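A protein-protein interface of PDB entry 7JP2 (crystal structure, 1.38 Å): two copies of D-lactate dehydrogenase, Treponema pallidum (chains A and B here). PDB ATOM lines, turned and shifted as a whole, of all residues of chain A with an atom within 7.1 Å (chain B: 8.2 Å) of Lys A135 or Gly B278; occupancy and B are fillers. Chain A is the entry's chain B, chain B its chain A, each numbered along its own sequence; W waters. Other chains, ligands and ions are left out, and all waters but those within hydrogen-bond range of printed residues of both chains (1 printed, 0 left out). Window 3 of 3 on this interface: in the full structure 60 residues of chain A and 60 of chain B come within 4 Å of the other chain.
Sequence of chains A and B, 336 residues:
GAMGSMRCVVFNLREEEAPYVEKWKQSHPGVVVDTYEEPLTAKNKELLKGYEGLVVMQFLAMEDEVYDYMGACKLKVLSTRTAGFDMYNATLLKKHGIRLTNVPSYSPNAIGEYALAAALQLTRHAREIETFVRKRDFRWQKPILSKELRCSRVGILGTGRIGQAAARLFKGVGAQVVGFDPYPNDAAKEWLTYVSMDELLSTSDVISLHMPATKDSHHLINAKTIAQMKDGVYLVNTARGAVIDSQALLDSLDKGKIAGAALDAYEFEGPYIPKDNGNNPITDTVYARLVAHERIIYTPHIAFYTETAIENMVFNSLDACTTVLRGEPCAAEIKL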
ATOM      1  N   GLU A 128     -26.933  17.173   2.176  1.00  0.00           N
ATOM      2  CA  GLU A 128     -26.021  17.530   3.252  1.00  0.00           C
ATOM      3  C   GLU A 128     -26.782  17.862   4.528  1.00  0.00           C
ATOM      4  O   GLU A 128     -26.368  17.470   5.626  1.00  0.00           O
ATOM      5  CB  GLU A 128     -25.155  18.701   2.787  1.00  0.00           C
ATOM      6  CG  GLU A 128     -24.242  18.373   1.586  1.00  0.00           C
ATOM      7  CD  GLU A 128     -24.981  18.180   0.236  1.00  0.00           C
ATOM      8  OE1 GLU A 128     -26.048  18.796  -0.015  1.00  0.00           O
ATOM      9  OE2 GLU A 128     -24.487  17.389  -0.597  1.00  0.00           O
ATOM     10  N   ILE A 129     -27.908  18.564   4.400  1.00  0.00           N
ATOM     11  CA  ILE A 129     -28.757  18.840   5.556  1.00  0.00           C
ATOM     12  C   ILE A 129     -29.294  17.541   6.147  1.00  0.00           C
ATOM     13  O   ILE A 129     -29.271  17.341   7.366  1.00  0.00           O
ATOM     14  CB  ILE A 129     -29.893  19.813   5.192  1.00  0.00           C
ATOM     15  CG1 ILE A 129     -29.329  21.190   4.838  1.00  0.00           C
ATOM     16  CG2 ILE A 129     -30.859  19.927   6.352  1.00  0.00           C
ATOM     17  CD1 ILE A 129     -30.303  22.096   4.104  1.00  0.00           C
ATOM     18  N   GLU A 130     -29.767  16.627   5.289  1.00  0.00           N
ATOM     19  CA  GLU A 130     -30.314  15.365   5.787  1.00  0.00           C
ATOM     20  C   GLU A 130     -29.248  14.558   6.517  1.00  0.00           C
ATOM     21  O   GLU A 130     -29.533  13.910   7.529  1.00  0.00           O
ATOM     22  CB  GLU A 130     -30.926  14.583   4.622  1.00  0.00           C
ATOM     23  CG  GLU A 130     -31.384  13.186   4.964  1.00  0.00           C
ATOM     24  CD  GLU A 130     -32.625  13.097   5.839  1.00  0.00           C
ATOM     25  OE1 GLU A 130     -33.216  14.122   6.218  1.00  0.00           O
ATOM     26  OE2 GLU A 130     -33.019  11.952   6.130  1.00  0.00           O
ATOM     27  N   THR A 131     -28.007  14.603   6.032  1.00  0.00           N
ATOM     28  CA  THR A 131     -26.918  13.911   6.717  1.00  0.00           C
ATOM     29  C   THR A 131     -26.676  14.495   8.106  1.00  0.00           C
ATOM     30  O   THR A 131     -26.473  13.748   9.068  1.00  0.00           O
ATOM     31  CB  THR A 131     -25.653  13.974   5.865  1.00  0.00           C
ATOM     32  OG1 THR A 131     -25.857  13.203   4.675  1.00  0.00           O
ATOM     33  CG2 THR A 131     -24.445  13.438   6.614  1.00  0.00           C
ATOM     34  N   PHE A 132     -26.693  15.827   8.234  1.00  0.00           N
ATOM     35  CA  PHE A 132     -26.574  16.434   9.559  1.00  0.00           C
ATOM     36  C   PHE A 132     -27.782  16.090  10.428  1.00  0.00           C
ATOM     37  O   PHE A 132     -27.627  15.759  11.610  1.00  0.00           O
ATOM     38  CB  PHE A 132     -26.384  17.946   9.445  1.00  0.00           C
ATOM     39  CG  PHE A 132     -25.008  18.362   9.016  1.00  0.00           C
ATOM     40  CD1 PHE A 132     -23.886  17.914   9.689  1.00  0.00           C
ATOM     41  CD2 PHE A 132     -24.841  19.211   7.943  1.00  0.00           C
ATOM     42  CE1 PHE A 132     -22.633  18.313   9.299  1.00  0.00           C
ATOM     43  CE2 PHE A 132     -23.586  19.611   7.548  1.00  0.00           C
ATOM     44  CZ  PHE A 132     -22.483  19.156   8.219  1.00  0.00           C
ATOM     45  N   VAL A 133     -28.988  16.125   9.854  1.00  0.00           N
ATOM     46  CA  VAL A 133     -30.186  15.777  10.619  1.00  0.00           C
ATOM     47  C   VAL A 133     -30.094  14.349  11.146  1.00  0.00           C
ATOM     48  O   VAL A 133     -30.464  14.070  12.296  1.00  0.00           O
ATOM     49  CB  VAL A 133     -31.445  16.002   9.760  1.00  0.00           C
ATOM     50  CG1 VAL A 133     -32.663  15.310  10.352  1.00  0.00           C
ATOM     51  CG2 VAL A 133     -31.708  17.498   9.595  1.00  0.00           C
ATOM     52  N   ARG A 134     -29.600  13.425  10.317  1.00  0.00           N
ATOM     53  CA  ARG A 134     -29.465  12.032  10.735  1.00  0.00           C
ATOM     54  C   ARG A 134     -28.618  11.915  11.996  1.00  0.00           C
ATOM     55  O   ARG A 134     -28.896  11.077  12.866  1.00  0.00           O
ATOM     56  CB  ARG A 134     -28.847  11.245   9.574  1.00  0.00           C
ATOM     57  CG  ARG A 134     -28.586   9.776   9.814  1.00  0.00           C
ATOM     58  CD  ARG A 134     -28.325   9.046   8.461  1.00  0.00           C
ATOM     59  NE  ARG A 134     -27.190   9.542   7.661  1.00  0.00           N
ATOM     60  CZ  ARG A 134     -27.255  10.213   6.499  1.00  0.00           C
ATOM     61  NH1 ARG A 134     -28.403  10.546   5.895  1.00  0.00           N
ATOM     62  NH2 ARG A 134     -26.123  10.562   5.908  1.00  0.00           N
ATOM     63  N   LYS A 135     -27.573  12.739  12.108  1.00  0.00           N
ATOM     64  CA  LYS A 135     -26.694  12.790  13.270  1.00  0.00           C
ATOM     65  C   LYS A 135     -27.240  13.673  14.389  1.00  0.00           C
ATOM     66  O   LYS A 135     -26.590  13.814  15.428  1.00  0.00           O
ATOM     67  CB  LYS A 135     -25.309  13.297  12.839  1.00  0.00           C
ATOM     68  CG  LYS A 135     -24.605  12.425  11.815  1.00  0.00           C
ATOM     69  CD  LYS A 135     -23.206  12.952  11.492  1.00  0.00           C
ATOM     70  CE  LYS A 135     -23.215  14.109  10.504  1.00  0.00           C
ATOM     71  NZ  LYS A 135     -21.840  14.476  10.035  1.00  0.00           N
ATOM     72  N   ARG A 136     -28.415  14.268  14.195  1.00  0.00           N
ATOM     73  CA  ARG A 136     -29.037  15.195  15.148  1.00  0.00           C
ATOM     74  C   ARG A 136     -28.203  16.461  15.339  1.00  0.00           C
ATOM     75  O   ARG A 136     -28.272  17.116  16.382  1.00  0.00           O
ATOM     76  CB  ARG A 136     -29.396  14.513  16.476  1.00  0.00           C
ATOM     77  CG  ARG A 136     -30.253  13.272  16.293  1.00  0.00           C
ATOM     78  CD  ARG A 136     -31.608  13.612  15.693  1.00  0.00           C
ATOM     79  NE  ARG A 136     -32.478  12.443  15.603  1.00  0.00           N
ATOM     80  CZ  ARG A 136     -32.759  11.765  14.494  1.00  0.00           C
ATOM     81  NH1 ARG A 136     -32.256  12.106  13.316  1.00  0.00           N
ATOM     82  NH2 ARG A 136     -33.575  10.738  14.576  1.00  0.00           N
ATOM     83  N   ASP A 137     -27.422  16.816  14.317  1.00  0.00           N
ATOM     84  CA  ASP A 137     -26.628  18.044  14.293  1.00  0.00           C
ATOM     85  C   ASP A 137     -27.484  19.103  13.611  1.00  0.00           C
ATOM     86  O   ASP A 137     -27.581  19.149  12.380  1.00  0.00           O
ATOM     87  CB  ASP A 137     -25.322  17.819  13.543  1.00  0.00           C
ATOM     88  CG  ASP A 137     -24.422  19.038  13.554  1.00  0.00           C
ATOM     89  OD1 ASP A 137     -24.839  20.088  14.091  1.00  0.00           O
ATOM     90  OD2 ASP A 137     -23.299  18.946  13.019  1.00  0.00           O
ATOM     91  N   PHE A 138     -28.132  19.939  14.415  1.00  0.00           N
ATOM     92  CA  PHE A 138     -29.086  20.921  13.923  1.00  0.00           C
ATOM     93  C   PHE A 138     -28.501  22.335  13.893  1.00  0.00           C
ATOM     94  O   PHE A 138     -29.247  23.321  13.959  1.00  0.00           O
ATOM     95  CB  PHE A 138     -30.350  20.906  14.784  1.00  0.00           C
ATOM     96  CG  PHE A 138     -31.132  19.603  14.771  1.00  0.00           C
ATOM     97  CD1 PHE A 138     -30.930  18.606  13.832  1.00  0.00           C
ATOM     98  CD2 PHE A 138     -32.108  19.403  15.734  1.00  0.00           C
ATOM     99  CE1 PHE A 138     -31.693  17.442  13.862  1.00  0.00           C
ATOM    100  CE2 PHE A 138     -32.860  18.245  15.766  1.00  0.00           C
ATOM    101  CZ  PHE A 138     -32.653  17.265  14.831  1.00  0.00           C
ATOM    102  N   GLN A 141     -24.689  25.949  10.098  1.00  0.00           N
ATOM    103  CA  GLN A 141     -23.269  25.842   9.814  1.00  0.00           C
ATOM    104  C   GLN A 141     -22.981  26.042   8.334  1.00  0.00           C
ATOM    105  O   GLN A 141     -23.771  25.671   7.464  1.00  0.00           O
ATOM    106  CB  GLN A 141     -22.705  24.513  10.321  1.00  0.00           C
ATOM    107  CG  GLN A 141     -23.421  23.289   9.834  1.00  0.00           C
ATOM    108  CD  GLN A 141     -22.805  22.051  10.431  1.00  0.00           C
ATOM    109  OE1 GLN A 141     -21.588  21.894  10.438  1.00  0.00           O
ATOM    110  NE2 GLN A 141     -23.645  21.177  10.971  1.00  0.00           N
ATOM    111  N   LYS B 275     -28.705  23.518  17.538  1.00  0.00           N
ATOM    112  CA  LYS B 275     -27.637  22.941  18.333  1.00  0.00           C
ATOM    113  C   LYS B 275     -27.237  21.587  17.777  1.00  0.00           C
ATOM    114  O   LYS B 275     -28.013  20.921  17.091  1.00  0.00           O
ATOM    115  CB  LYS B 275     -28.108  22.780  19.778  1.00  0.00           C
ATOM    116  CG  LYS B 275     -28.467  24.114  20.380  1.00  0.00           C
ATOM    117  CD  LYS B 275     -28.480  24.070  21.877  1.00  0.00           C
ATOM    118  CE  LYS B 275     -29.580  23.179  22.373  1.00  0.00           C
ATOM    119  NZ  LYS B 275     -30.064  23.652  23.711  1.00  0.00           N
ATOM    120  N   ASP B 276     -26.006  21.183  18.080  1.00  0.00           N
ATOM    121  CA  ASP B 276     -25.556  19.827  17.804  1.00  0.00           C
ATOM    122  C   ASP B 276     -26.031  18.948  18.952  1.00  0.00           C
ATOM    123  O   ASP B 276     -25.540  19.070  20.078  1.00  0.00           O
ATOM    124  CB  ASP B 276     -24.039  19.777  17.666  1.00  0.00           C
ATOM    125  CG  ASP B 276     -23.530  18.380  17.361  1.00  0.00           C
ATOM    126  OD1 ASP B 276     -24.347  17.449  17.235  1.00  0.00           O
ATOM    127  OD2 ASP B 276     -22.300  18.213  17.264  1.00  0.00           O
ATOM    128  N   ASN B 277     -26.985  18.062  18.669  1.00  0.00           N
ATOM    129  CA  ASN B 277     -27.580  17.203  19.682  1.00  0.00           C
ATOM    130  C   ASN B 277     -27.061  15.777  19.612  1.00  0.00           C
ATOM    131  O   ASN B 277     -27.701  14.865  20.141  1.00  0.00           O
ATOM    132  CB  ASN B 277     -29.100  17.232  19.555  1.00  0.00           C
ATOM    133  CG  ASN B 277     -29.651  18.635  19.662  1.00  0.00           C
ATOM    134  OD1 ASN B 277     -29.594  19.236  20.720  1.00  0.00           O
ATOM    135  ND2 ASN B 277     -30.172  19.170  18.561  1.00  0.00           N
ATOM    136  N   GLY B 278     -25.899  15.572  18.998  1.00  0.00           N
ATOM    137  CA  GLY B 278     -25.347  14.231  18.915  1.00  0.00           C
ATOM    138  C   GLY B 278     -25.210  13.543  20.256  1.00  0.00           C
ATOM    139  O   GLY B 278     -25.314  12.315  20.340  1.00  0.00           O
ATOM    140  N   ASN B 279     -24.940  14.306  21.314  1.00  0.00           N
ATOM    141  CA  ASN B 279     -24.852  13.763  22.663  1.00  0.00           C
ATOM    142  C   ASN B 279     -25.867  14.431  23.583  1.00  0.00           C
ATOM    143  O   ASN B 279     -25.629  14.600  24.784  1.00  0.00           O
ATOM    144  CB  ASN B 279     -23.440  13.880  23.225  1.00  0.00           C
ATOM    145  CG  ASN B 279     -23.221  12.975  24.427  1.00  0.00           C
ATOM    146  OD1 ASN B 279     -23.744  11.852  24.493  1.00  0.00           O
ATOM    147  ND2 ASN B 279     -22.457  13.465  25.394  1.00  0.00           N
ATOM    148  N   ASN B 280     -27.022  14.787  23.022  1.00  0.00           N
ATOM    149  CA  ASN B 280     -28.096  15.445  23.762  1.00  0.00           C
ATOM    150  C   ASN B 280     -29.397  14.795  23.317  1.00  0.00           C
ATOM    151  O   ASN B 280     -30.031  15.233  22.349  1.00  0.00           O
ATOM    152  CB  ASN B 280     -28.114  16.942  23.473  1.00  0.00           C
ATOM    153  CG  ASN B 280     -29.157  17.669  24.274  1.00  0.00           C
ATOM    154  OD1 ASN B 280     -29.336  17.394  25.459  1.00  0.00           O
ATOM    155  ND2 ASN B 280     -29.858  18.601  23.635  1.00  0.00           N
ATOM    156  N   PRO B 281     -29.815  13.728  23.989  1.00  0.00           N
ATOM    157  CA  PRO B 281     -30.990  12.983  23.521  1.00  0.00           C
ATOM    158  C   PRO B 281     -32.232  13.851  23.434  1.00  0.00           C
ATOM    159  O   PRO B 281     -32.503  14.676  24.308  1.00  0.00           O
ATOM    160  CB  PRO B 281     -31.154  11.890  24.586  1.00  0.00           C
ATOM    161  CG  PRO B 281     -29.777  11.667  25.076  1.00  0.00           C
ATOM    162  CD  PRO B 281     -29.141  13.039  25.103  1.00  0.00           C
ATOM    163  N   ILE B 282     -33.001  13.652  22.377  1.00  0.00           N
ATOM    164  CA  ILE B 282     -34.306  14.289  22.284  1.00  0.00           C
ATOM    165  C   ILE B 282     -35.250  13.552  23.223  1.00  0.00           C
ATOM    166  O   ILE B 282     -35.530  12.364  23.035  1.00  0.00           O
ATOM    167  CB  ILE B 282     -34.823  14.297  20.833  1.00  0.00           C
ATOM    168  CG1 ILE B 282     -33.908  15.168  19.956  1.00  0.00           C
ATOM    169  CG2 ILE B 282     -36.254  14.812  20.785  1.00  0.00           C
ATOM    170  CD1 ILE B 282     -34.189  15.093  18.464  1.00  0.00           C
HETATM  171  O   HOH W   1     -24.065  15.073  15.848  1.00  0.00           O
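Lys A135 touches Gly B278. Arg A136 touches Lys B275. C of Asp B276 touches O of Arg A136, 3.9 Å away. Gly B278 touches Arg A136 (N to O, 3.9 Å). C of Asp A137 touches O of Lys B275 (3.96 Å). Asp A137 touches Asp B276. Asn B277 touches Phe A138.
The side-chain amide oxygen (OD1) of Asn B277 is in hydrogen-bond range of the side-chain amide nitrogen (ND2) of Asn B280 (3.0 Å). The side-chain amide nitrogen (ND2) of Asn B277 is in hydrogen-bond range of the backbone carbonyl oxygen (O) of Lys B275 (3.1 Å). The backbone NH of Asp A137 sits at hydrogen-bond distance from the backbone carbonyl oxygen of Phe A132, 2.9 Å away. The side-chain amide nitrogen (NE2) of Gln A141 lies within hydrogen-bond range of the side-chain carboxylate (OD2) of Asp A137 (3.0 Å). OD1 of Asp B276 sits at hydrogen-bond distance from N of Gly B278 (3.0 Å). The backbone carbonyl oxygen (O) of Val A133 sits at hydrogen-bond distance from the guanidinium group (NH1) of Arg A136, 2.8 Å away.
Water W1 bridges the side-chain carboxylate of Asp B276 (2.8 Å) and the backbone carbonyl oxygen of Lys A135 (2.9 Å).
No position is printed for both chains. Of the 9 pairs that touch across the chains among the printed residues, none has its exchanged pair printed and touching as well.
Ile A129 touches none of the printed residues of chain B. Lys A135 touches just one residue of chain B: Gly B278 (3.7 Å). Printed residues of chain B within 4 Å of Arg A136: Lys B275, Asp B276, Asn B277 and Gly B278. Of the printed residues of chain B, Asp A137 touches Lys B275 and Asp B276. Of the printed residues of chain B, Phe A138 touches Lys B275 (2.9 Å) and Asn B277 (3.4 Å). Printed residues of chain A within 4 Å of Lys B275: Arg A136 (3.9 Å), Asp A137 (3.96 Å) and Phe A138 (2.9 Å). Gly B278 touches just these residues of chain A: Lys A135 and Arg A136. Ile B282 touches none of the printed residues of chain A. The nearest printed residue of chain B that does not touch Lys A135 is Asp B276 (4.6 Å). The nearest residue of chain A that does not touch Gly B278 is Asp A137 (5.1 Å).
The backbone NH of Asn B277 is in hydrogen-bond range of the backbone carbonyl oxygen of Arg A136. O of Lys B275 sits at hydrogen-bond distance from N of Phe A138, at 2.9 Å.
Hydrophobic or aromatic side chains of chain A that line the printed part of chain B: Phe A138.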
